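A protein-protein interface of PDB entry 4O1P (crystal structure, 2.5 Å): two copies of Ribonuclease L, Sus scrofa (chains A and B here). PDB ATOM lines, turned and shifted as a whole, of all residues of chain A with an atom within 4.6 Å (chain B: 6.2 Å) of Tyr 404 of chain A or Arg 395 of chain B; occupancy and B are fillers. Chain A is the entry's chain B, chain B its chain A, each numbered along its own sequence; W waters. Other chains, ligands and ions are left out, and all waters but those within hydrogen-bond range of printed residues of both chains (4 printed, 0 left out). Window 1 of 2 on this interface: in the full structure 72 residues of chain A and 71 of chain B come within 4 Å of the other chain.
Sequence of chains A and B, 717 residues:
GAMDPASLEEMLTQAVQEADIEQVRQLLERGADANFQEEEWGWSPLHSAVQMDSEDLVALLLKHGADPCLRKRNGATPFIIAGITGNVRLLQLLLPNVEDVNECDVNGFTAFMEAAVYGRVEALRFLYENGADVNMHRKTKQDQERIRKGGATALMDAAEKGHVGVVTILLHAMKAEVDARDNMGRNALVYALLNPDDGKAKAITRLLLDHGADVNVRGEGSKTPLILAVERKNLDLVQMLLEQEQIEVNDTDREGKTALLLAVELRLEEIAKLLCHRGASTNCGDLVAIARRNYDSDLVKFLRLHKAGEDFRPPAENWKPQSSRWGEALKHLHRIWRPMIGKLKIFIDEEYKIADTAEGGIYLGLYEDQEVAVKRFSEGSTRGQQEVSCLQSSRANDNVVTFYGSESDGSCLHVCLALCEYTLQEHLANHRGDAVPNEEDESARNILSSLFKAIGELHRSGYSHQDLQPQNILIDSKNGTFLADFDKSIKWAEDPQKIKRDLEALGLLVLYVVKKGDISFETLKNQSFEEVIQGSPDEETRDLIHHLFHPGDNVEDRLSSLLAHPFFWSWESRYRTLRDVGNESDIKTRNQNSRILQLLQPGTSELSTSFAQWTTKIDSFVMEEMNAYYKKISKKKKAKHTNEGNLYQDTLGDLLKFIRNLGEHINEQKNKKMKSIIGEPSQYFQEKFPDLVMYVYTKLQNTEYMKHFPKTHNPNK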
ATOM      1  N   TYR A 367      -1.763  -2.620 -21.085  1.00  0.00           N
ATOM      2  CA  TYR A 367      -0.824  -3.192 -20.120  1.00  0.00           C
ATOM      3  C   TYR A 367      -0.265  -4.457 -20.741  1.00  0.00           C
ATOM      4  O   TYR A 367      -1.026  -5.353 -21.063  1.00  0.00           O
ATOM      5  CB  TYR A 367      -1.563  -3.515 -18.825  1.00  0.00           C
ATOM      6  CG  TYR A 367      -0.708  -4.101 -17.720  1.00  0.00           C
ATOM      7  CD1 TYR A 367      -0.361  -5.435 -17.728  1.00  0.00           C
ATOM      8  CD2 TYR A 367      -0.269  -3.313 -16.657  1.00  0.00           C
ATOM      9  CE1 TYR A 367       0.409  -5.983 -16.716  1.00  0.00           C
ATOM     10  CE2 TYR A 367       0.518  -3.844 -15.641  1.00  0.00           C
ATOM     11  CZ  TYR A 367       0.840  -5.187 -15.664  1.00  0.00           C
ATOM     12  OH  TYR A 367       1.612  -5.752 -14.665  1.00  0.00           O
ATOM     13  N   GLU A 368       1.053  -4.523 -20.918  1.00  0.00           N
ATOM     14  CA  GLU A 368       1.683  -5.612 -21.673  1.00  0.00           C
ATOM     15  C   GLU A 368       0.957  -5.791 -23.013  1.00  0.00           C
ATOM     16  O   GLU A 368       0.687  -6.917 -23.448  1.00  0.00           O
ATOM     17  CB  GLU A 368       1.698  -6.924 -20.849  1.00  0.00           C
ATOM     18  CG  GLU A 368       2.661  -6.904 -19.655  1.00  0.00           C
ATOM     19  CD  GLU A 368       2.480  -8.070 -18.657  1.00  0.00           C
ATOM     20  OE1 GLU A 368       1.413  -8.749 -18.629  1.00  0.00           O
ATOM     21  OE2 GLU A 368       3.412  -8.290 -17.851  1.00  0.00           O
ATOM     22  N   GLN A 370      -2.103  -5.387 -23.693  1.00  0.00           N
ATOM     23  CA  GLN A 370      -3.471  -5.854 -23.515  1.00  0.00           C
ATOM     24  C   GLN A 370      -4.342  -4.671 -23.145  1.00  0.00           C
ATOM     25  O   GLN A 370      -3.932  -3.832 -22.344  1.00  0.00           O
ATOM     26  CB  GLN A 370      -3.542  -6.900 -22.398  1.00  0.00           C
ATOM     27  CG  GLN A 370      -2.548  -8.035 -22.528  1.00  0.00           C
ATOM     28  CD  GLN A 370      -2.581  -8.682 -23.898  1.00  0.00           C
ATOM     29  OE1 GLN A 370      -1.572  -8.721 -24.603  1.00  0.00           O
ATOM     30  NE2 GLN A 370      -3.747  -9.187 -24.283  1.00  0.00           N
ATOM     31  N   VAL A 372      -6.967  -2.668 -21.129  1.00  0.00           N
ATOM     32  CA  VAL A 372      -7.366  -2.713 -19.709  1.00  0.00           C
ATOM     33  C   VAL A 372      -8.156  -1.478 -19.290  1.00  0.00           C
ATOM     34  O   VAL A 372      -8.147  -0.459 -19.978  1.00  0.00           O
ATOM     35  CB  VAL A 372      -6.157  -2.806 -18.747  1.00  0.00           C
ATOM     36  CG1 VAL A 372      -5.479  -4.153 -18.875  1.00  0.00           C
ATOM     37  CG2 VAL A 372      -5.160  -1.697 -19.006  1.00  0.00           C
ATOM     38  N   ARG A 395      -6.616 -13.779  -7.658  1.00  0.00           N
ATOM     39  CA  ARG A 395      -6.309 -14.094  -9.060  1.00  0.00           C
ATOM     40  C   ARG A 395      -6.883 -15.421  -9.535  1.00  0.00           C
ATOM     41  O   ARG A 395      -7.233 -15.547 -10.704  1.00  0.00           O
ATOM     42  CB  ARG A 395      -4.801 -14.065  -9.318  1.00  0.00           C
ATOM     43  CG  ARG A 395      -4.191 -12.692  -9.137  1.00  0.00           C
ATOM     44  CD  ARG A 395      -2.708 -12.669  -9.460  1.00  0.00           C
ATOM     45  NE  ARG A 395      -2.470 -11.840 -10.627  1.00  0.00           N
ATOM     46  CZ  ARG A 395      -1.759 -10.721 -10.669  1.00  0.00           C
ATOM     47  NH1 ARG A 395      -1.127 -10.245  -9.609  1.00  0.00           N
ATOM     48  NH2 ARG A 395      -1.654 -10.093 -11.825  1.00  0.00           N
ATOM     49  N   THR A 402     -10.613  -9.789 -13.791  1.00  0.00           N
ATOM     50  CA  THR A 402      -9.255 -10.257 -13.891  1.00  0.00           C
ATOM     51  C   THR A 402      -8.295  -9.098 -13.641  1.00  0.00           C
ATOM     52  O   THR A 402      -8.377  -8.048 -14.270  1.00  0.00           O
ATOM     53  CB  THR A 402      -8.993 -10.923 -15.261  1.00  0.00           C
ATOM     54  OG1 THR A 402      -9.829 -12.079 -15.396  1.00  0.00           O
ATOM     55  CG2 THR A 402      -7.547 -11.356 -15.402  1.00  0.00           C
ATOM     56  N   PHE A 403      -7.378  -9.332 -12.711  1.00  0.00           N
ATOM     57  CA  PHE A 403      -6.374  -8.382 -12.305  1.00  0.00           C
ATOM     58  C   PHE A 403      -5.127  -8.611 -13.142  1.00  0.00           C
ATOM     59  O   PHE A 403      -4.579  -9.718 -13.170  1.00  0.00           O
ATOM     60  CB  PHE A 403      -6.076  -8.612 -10.827  1.00  0.00           C
ATOM     61  CG  PHE A 403      -5.006  -7.737 -10.261  1.00  0.00           C
ATOM     62  CD1 PHE A 403      -5.010  -6.371 -10.482  1.00  0.00           C
ATOM     63  CD2 PHE A 403      -4.013  -8.279  -9.449  1.00  0.00           C
ATOM     64  CE1 PHE A 403      -4.035  -5.557  -9.927  1.00  0.00           C
ATOM     65  CE2 PHE A 403      -3.018  -7.463  -8.896  1.00  0.00           C
ATOM     66  CZ  PHE A 403      -3.036  -6.101  -9.138  1.00  0.00           C
ATOM     67  N   TYR A 404      -4.663  -7.552 -13.805  1.00  0.00           N
ATOM     68  CA  TYR A 404      -3.438  -7.610 -14.560  1.00  0.00           C
ATOM     69  C   TYR A 404      -2.244  -7.259 -13.671  1.00  0.00           C
ATOM     70  O   TYR A 404      -1.233  -7.958 -13.657  1.00  0.00           O
ATOM     71  CB  TYR A 404      -3.544  -6.705 -15.809  1.00  0.00           C
ATOM     72  CG  TYR A 404      -4.287  -7.371 -16.959  1.00  0.00           C
ATOM     73  CD1 TYR A 404      -5.611  -7.717 -16.844  1.00  0.00           C
ATOM     74  CD2 TYR A 404      -3.642  -7.682 -18.148  1.00  0.00           C
ATOM     75  CE1 TYR A 404      -6.290  -8.345 -17.879  1.00  0.00           C
ATOM     76  CE2 TYR A 404      -4.308  -8.313 -19.190  1.00  0.00           C
ATOM     77  CZ  TYR A 404      -5.629  -8.644 -19.051  1.00  0.00           C
ATOM     78  OH  TYR A 404      -6.304  -9.272 -20.086  1.00  0.00           O
ATOM     79  N   GLY A 405      -2.341  -6.159 -12.948  1.00  0.00           N
ATOM     80  CA  GLY A 405      -1.242  -5.704 -12.087  1.00  0.00           C
ATOM     81  C   GLY A 405      -1.404  -4.238 -11.749  1.00  0.00           C
ATOM     82  O   GLY A 405      -2.398  -3.621 -12.136  1.00  0.00           O
ATOM     83  N   CYS A 416      -4.664  -1.927 -12.836  1.00  0.00           N
ATOM     84  CA  CYS A 416      -5.084  -2.353 -14.172  1.00  0.00           C
ATOM     85  C   CYS A 416      -5.935  -3.625 -14.148  1.00  0.00           C
ATOM     86  O   CYS A 416      -5.492  -4.675 -13.663  1.00  0.00           O
ATOM     87  CB  CYS A 416      -3.860  -2.604 -15.031  1.00  0.00           C
ATOM     88  SG  CYS A 416      -2.774  -1.168 -15.142  1.00  0.00           S
ATOM     89  N   LEU A 417      -7.125  -3.526 -14.733  1.00  0.00           N
ATOM     90  CA  LEU A 417      -8.120  -4.587 -14.712  1.00  0.00           C
ATOM     91  C   LEU A 417      -8.554  -4.982 -16.133  1.00  0.00           C
ATOM     92  O   LEU A 417      -8.436  -4.188 -17.059  1.00  0.00           O
ATOM     93  CB  LEU A 417      -9.358  -4.093 -13.975  1.00  0.00           C
ATOM     94  CG  LEU A 417      -9.161  -3.440 -12.610  1.00  0.00           C
ATOM     95  CD1 LEU A 417     -10.439  -2.768 -12.136  1.00  0.00           C
ATOM     96  CD2 LEU A 417      -8.712  -4.464 -11.597  1.00  0.00           C
ATOM     97  N   ALA A 418      -9.076  -6.195 -16.292  1.00  0.00           N
ATOM     98  CA  ALA A 418      -9.737  -6.593 -17.543  1.00  0.00           C
ATOM     99  C   ALA A 418     -10.814  -5.579 -17.926  1.00  0.00           C
ATOM    100  O   ALA A 418     -11.590  -5.145 -17.096  1.00  0.00           O
ATOM    101  CB  ALA A 418     -10.351  -7.974 -17.404  1.00  0.00           C
ATOM    102  N   TYR B 367       5.095 -14.327  -4.884  1.00  0.00           N
ATOM    103  CA  TYR B 367       4.955 -13.167  -5.766  1.00  0.00           C
ATOM    104  C   TYR B 367       3.818 -12.343  -5.211  1.00  0.00           C
ATOM    105  O   TYR B 367       2.711 -12.841  -5.097  1.00  0.00           O
ATOM    106  CB  TYR B 367       4.629 -13.641  -7.196  1.00  0.00           C
ATOM    107  CG  TYR B 367       4.458 -12.553  -8.214  1.00  0.00           C
ATOM    108  CD1 TYR B 367       3.286 -11.815  -8.277  1.00  0.00           C
ATOM    109  CD2 TYR B 367       5.473 -12.230  -9.091  1.00  0.00           C
ATOM    110  CE1 TYR B 367       3.122 -10.797  -9.217  1.00  0.00           C
ATOM    111  CE2 TYR B 367       5.317 -11.224 -10.034  1.00  0.00           C
ATOM    112  CZ  TYR B 367       4.140 -10.509 -10.089  1.00  0.00           C
ATOM    113  OH  TYR B 367       3.970  -9.495 -11.016  1.00  0.00           O
ATOM    114  N   CYS B 390       2.524 -15.580 -24.837  1.00  0.00           N
ATOM    115  CA  CYS B 390       1.248 -16.291 -24.838  1.00  0.00           C
ATOM    116  C   CYS B 390       0.467 -16.103 -23.532  1.00  0.00           C
ATOM    117  O   CYS B 390      -0.742 -15.851 -23.537  1.00  0.00           O
ATOM    118  CB  CYS B 390       1.495 -17.764 -25.097  1.00  0.00           C
ATOM    119  SG  CYS B 390      -0.014 -18.721 -25.181  1.00  0.00           S
ATOM    120  N   LEU B 391       1.160 -16.201 -22.408  1.00  0.00           N
ATOM    121  CA  LEU B 391       0.531 -15.958 -21.102  1.00  0.00           C
ATOM    122  C   LEU B 391      -0.022 -14.540 -20.957  1.00  0.00           C
ATOM    123  O   LEU B 391      -1.075 -14.345 -20.374  1.00  0.00           O
ATOM    124  CB  LEU B 391       1.530 -16.254 -19.979  1.00  0.00           C
ATOM    125  CG  LEU B 391       1.817 -17.746 -19.811  1.00  0.00           C
ATOM    126  CD1 LEU B 391       3.110 -17.989 -19.048  1.00  0.00           C
ATOM    127  CD2 LEU B 391       0.665 -18.437 -19.116  1.00  0.00           C
ATOM    128  N   GLN B 392       0.692 -13.550 -21.485  1.00  0.00           N
ATOM    129  CA  GLN B 392       0.228 -12.151 -21.452  1.00  0.00           C
ATOM    130  C   GLN B 392      -1.097 -11.936 -22.164  1.00  0.00           C
ATOM    131  O   GLN B 392      -1.840 -11.014 -21.803  1.00  0.00           O
ATOM    132  CB  GLN B 392       1.281 -11.219 -22.043  1.00  0.00           C
ATOM    133  CG  GLN B 392       2.401 -10.925 -21.069  1.00  0.00           C
ATOM    134  CD  GLN B 392       3.580 -10.208 -21.696  1.00  0.00           C
ATOM    135  OE1 GLN B 392       3.632 -10.001 -22.905  1.00  0.00           O
ATOM    136  NE2 GLN B 392       4.552  -9.845 -20.863  1.00  0.00           N
ATOM    137  N   SER B 393      -1.378 -12.752 -23.184  1.00  0.00           N
ATOM    138  CA  SER B 393      -2.642 -12.670 -23.933  1.00  0.00           C
ATOM    139  C   SER B 393      -3.738 -13.607 -23.437  1.00  0.00           C
ATOM    140  O   SER B 393      -4.829 -13.597 -23.992  1.00  0.00           O
ATOM    141  CB  SER B 393      -2.400 -12.997 -25.412  1.00  0.00           C
ATOM    142  OG  SER B 393      -1.479 -12.096 -25.983  1.00  0.00           O
ATOM    143  N   SER B 394      -3.457 -14.411 -22.415  1.00  0.00           N
ATOM    144  CA  SER B 394      -4.370 -15.460 -21.994  1.00  0.00           C
ATOM    145  C   SER B 394      -4.970 -15.274 -20.588  1.00  0.00           C
ATOM    146  O   SER B 394      -5.574 -16.192 -20.055  1.00  0.00           O
ATOM    147  CB  SER B 394      -3.668 -16.806 -22.097  1.00  0.00           C
ATOM    148  OG  SER B 394      -3.397 -17.116 -23.465  1.00  0.00           O
ATOM    149  N   ARG B 395      -4.860 -14.077 -20.019  1.00  0.00           N
ATOM    150  CA  ARG B 395      -5.293 -13.855 -18.641  1.00  0.00           C
ATOM    151  C   ARG B 395      -6.800 -14.043 -18.441  1.00  0.00           C
ATOM    152  O   ARG B 395      -7.220 -14.431 -17.350  1.00  0.00           O
ATOM    153  CB  ARG B 395      -4.870 -12.461 -18.144  1.00  0.00           C
ATOM    154  CG  ARG B 395      -3.376 -12.284 -18.084  1.00  0.00           C
ATOM    155  CD  ARG B 395      -2.963 -10.929 -17.547  1.00  0.00           C
ATOM    156  NE  ARG B 395      -2.283 -11.088 -16.267  1.00  0.00           N
ATOM    157  CZ  ARG B 395      -1.027 -10.763 -15.995  1.00  0.00           C
ATOM    158  NH1 ARG B 395      -0.238 -10.191 -16.888  1.00  0.00           N
ATOM    159  NH2 ARG B 395      -0.571 -11.012 -14.790  1.00  0.00           N
ATOM    160  N   ALA B 396      -7.601 -13.768 -19.480  1.00  0.00           N
ATOM    161  CA  ALA B 396      -9.052 -14.029 -19.438  1.00  0.00           C
ATOM    162  C   ALA B 396      -9.417 -15.503 -19.635  1.00  0.00           C
ATOM    163  O   ALA B 396     -10.583 -15.875 -19.458  1.00  0.00           O
ATOM    164  CB  ALA B 396      -9.787 -13.184 -20.477  1.00  0.00           C
ATOM    165  N   ASN B 397      -8.447 -16.342 -20.002  1.00  0.00           N
ATOM    166  CA  ASN B 397      -8.713 -17.757 -20.266  1.00  0.00           C
ATOM    167  C   ASN B 397      -8.717 -18.558 -18.969  1.00  0.00           C
ATOM    168  O   ASN B 397      -7.676 -18.889 -18.439  1.00  0.00           O
ATOM    169  CB  ASN B 397      -7.684 -18.312 -21.257  1.00  0.00           C
ATOM    170  CG  ASN B 397      -8.012 -19.715 -21.721  1.00  0.00           C
ATOM    171  OD1 ASN B 397      -8.699 -20.456 -21.029  1.00  0.00           O
ATOM    172  ND2 ASN B 397      -7.498 -20.098 -22.875  1.00  0.00           N
ATOM    173  N   ASP B 398      -9.906 -18.864 -18.458  1.00  0.00           N
ATOM    174  CA  ASP B 398     -10.068 -19.489 -17.125  1.00  0.00           C
ATOM    175  C   ASP B 398      -9.438 -20.869 -17.032  1.00  0.00           C
ATOM    176  O   ASP B 398      -9.126 -21.340 -15.946  1.00  0.00           O
ATOM    177  CB  ASP B 398     -11.561 -19.605 -16.751  1.00  0.00           C
ATOM    178  CG  ASP B 398     -12.223 -18.236 -16.510  1.00  0.00           C
ATOM    179  OD1 ASP B 398     -11.503 -17.231 -16.276  1.00  0.00           O
ATOM    180  OD2 ASP B 398     -13.471 -18.158 -16.526  1.00  0.00           O
ATOM    181  N   PHE B 403      -1.649 -16.700 -14.679  1.00  0.00           N
ATOM    182  CA  PHE B 403      -0.393 -16.002 -14.842  1.00  0.00           C
ATOM    183  C   PHE B 403      -0.346 -14.824 -13.869  1.00  0.00           C
ATOM    184  O   PHE B 403      -1.254 -13.996 -13.859  1.00  0.00           O
ATOM    185  CB  PHE B 403      -0.308 -15.504 -16.279  1.00  0.00           C
ATOM    186  CG  PHE B 403       0.919 -14.693 -16.593  1.00  0.00           C
ATOM    187  CD1 PHE B 403       2.175 -15.137 -16.231  1.00  0.00           C
ATOM    188  CD2 PHE B 403       0.813 -13.509 -17.313  1.00  0.00           C
ATOM    189  CE1 PHE B 403       3.295 -14.399 -16.544  1.00  0.00           C
ATOM    190  CE2 PHE B 403       1.930 -12.765 -17.613  1.00  0.00           C
ATOM    191  CZ  PHE B 403       3.176 -13.207 -17.226  1.00  0.00           C
ATOM    192  N   TYR B 404       0.686 -14.780 -13.029  1.00  0.00           N
ATOM    193  CA  TYR B 404       0.852 -13.694 -12.081  1.00  0.00           C
ATOM    194  C   TYR B 404       1.676 -12.570 -12.725  1.00  0.00           C
ATOM    195  O   TYR B 404       1.289 -11.405 -12.695  1.00  0.00           O
ATOM    196  CB  TYR B 404       1.478 -14.206 -10.783  1.00  0.00           C
ATOM    197  CG  TYR B 404       0.456 -14.836  -9.835  1.00  0.00           C
ATOM    198  CD1 TYR B 404      -0.212 -15.991 -10.181  1.00  0.00           C
ATOM    199  CD2 TYR B 404       0.167 -14.270  -8.610  1.00  0.00           C
ATOM    200  CE1 TYR B 404      -1.144 -16.565  -9.335  1.00  0.00           C
ATOM    201  CE2 TYR B 404      -0.756 -14.837  -7.752  1.00  0.00           C
ATOM    202  CZ  TYR B 404      -1.412 -15.984  -8.125  1.00  0.00           C
ATOM    203  OH  TYR B 404      -2.323 -16.560  -7.284  1.00  0.00           O
ATOM    204  N   GLY B 405       2.781 -12.929 -13.359  1.00  0.00           N
ATOM    205  CA  GLY B 405       3.636 -11.940 -14.005  1.00  0.00           C
ATOM    206  C   GLY B 405       5.013 -12.492 -14.215  1.00  0.00           C
ATOM    207  O   GLY B 405       5.256 -13.662 -13.921  1.00  0.00           O
HETATM  208  O   HOH W   1      -3.059 -10.555 -27.329  1.00  0.00           O
HETATM  209  O   HOH W   2      -4.466 -11.436 -21.223  1.00  0.00           O
HETATM  210  O   HOH W   3      -0.850  -9.523 -19.460  1.00  0.00           O
HETATM  211  O   HOH W   4      -4.112 -14.317  -6.178  1.00  0.00           O
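The backbone carbonyl oxygen (O) of Tyr 404 of chain B sits at hydrogen-bond distance from the guanidinium group (NH2) of Arg 395 of chain A (3.3 Å).
NH2 of Arg 395 of chain A sits close to NH2 of Arg 395 of chain B (3.3 Å).
NH1 of Arg 395 of chain B is in salt-bridge range of OE1 of Glu 368 of chain A, at 2.8 Å.
NH2 of Arg 395 of chain B is in hydrogen-bond range of O of Tyr 404 of chain A, 3.3 Å away.
The backbone carbonyl oxygen of Glu 368 of chain A lies close to the side-chain amide oxygen of Gln 370 of chain A (3.1 Å).
O of Thr 402 of chain A lies within hydrogen-bond range of N of Ala 418 of chain A, 2.8 Å away.
O of Phe 403 of chain B sits at hydrogen-bond distance from NH2 of Arg 395 of chain B (3.2 Å).
The backbone NH (N) of Tyr 404 of chain A lies within hydrogen-bond range of the backbone carbonyl oxygen (O) of Cys 416 of chain A (3.0 Å).
The guanidinium group of Arg 395 of chain A is in hydrogen-bond range of the backbone carbonyl oxygen of Tyr 404 of chain A (2.8 Å).
The guanidinium group of Arg 395 of chain B lies within hydrogen-bond range of the backbone carbonyl oxygen of Tyr 404 of chain B (2.8 Å).
Gln 392 of chain B touches Glu 368 of chain A (CG to OE1, 3.4 Å).
Gln 370 of chain A touches Gln 392 of chain B.
OE1 of Gln 370 of chain A touches OG of Ser 393 of chain B, 3.6 Å away.
Thr 402 of chain A touches Arg 395 of chain B.
Of chain B, only Arg 395 (3.3 Å) comes within 4 Å of Tyr 404 of chain A.
Of chain A, only Glu 368 (2.8 Å), Arg 395 (3.3 Å), Thr 402 (3.7 Å) and Tyr 404 (3.3 Å) come within 4 Å of Arg 395 of chain B.
Printed residues of chain A within 4 Å of Tyr 404 of chain B: Arg 395.
Of the printed residues of chain A, Gln 392 of chain B touches Glu 368 (3.4 Å) and Gln 370 (3.1 Å).
Of the printed residues of chain B, Thr 402 of chain A touches Arg 395 (3.7 Å).
Of the printed residues of chain B, Glu 368 of chain A touches Gln 392 (3.4 Å) and Arg 395 (2.8 Å).
Printed residues of chain B within 4 Å of Gln 370 of chain A: Gln 392 and Ser 393.
Ala 396 of chain B touches none of the printed residues of chain A.
The nearest residue of chain B that does not touch Tyr 404 of chain A is Tyr 404 of chain B (4.4 Å).
The nearest residue of chain A that does not touch Arg 395 of chain B is Phe 403 of chain A (4.1 Å).
Of the 13 printed residues of chain B, 4 touch a printed residue of chain A.
Hydrophobic or aromatic side chains of chain B within 4 Å of the printed part of chain A: Tyr 404.
Of the 12 printed residues of chain A, 5 touch a printed residue of chain B.
Among the printed residues, 8 pairs touch across the chains.
Among the printed residues, Asp or Glu carboxylates within 4 Å of a Lys or Arg side-chain nitrogen of the other chain: Glu 368 of chain A with Arg 395 of chain B.
Arg 395 of chain A touches its own counterpart, Arg 395 of chain B.
Arg 395 of chain A touches Tyr 404 of chain B, and with the chains exchanged Tyr 404 of chain A touches Arg 395 of chain B.
5 positions are printed for both chains.
Of the 8 pairs that touch across the chains among the printed residues, 3 have their exchanged pair printed and touching as well.
Water W3 lies within hydrogen-bond range of OE1 of Glu 368 of chain A (2.5 Å), NH1 of Arg 395 of chain B (2.7 Å) and O of Gln 392 of chain B (2.9 Å).
Water W1 bridges the side-chain hydroxyl (OG) of Ser 393 of chain B (2.6 Å) and the side-chain amide nitrogen (NE2) of Gln 370 of chain A (3.4 Å).
Water W2 lies within hydrogen-bond range of O of Gln 392 of chain B (2.7 Å), N of Arg 395 of chain B (2.9 Å), OH of Tyr 404 of chain A (3.1 Å) and N of Ser 394 of chain B (3.4 Å).
Water W4 bridges the backbone NH of Arg 395 of chain A (3.0 Å) and the side-chain hydroxyl of Tyr 404 of chain B (3.1 Å).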
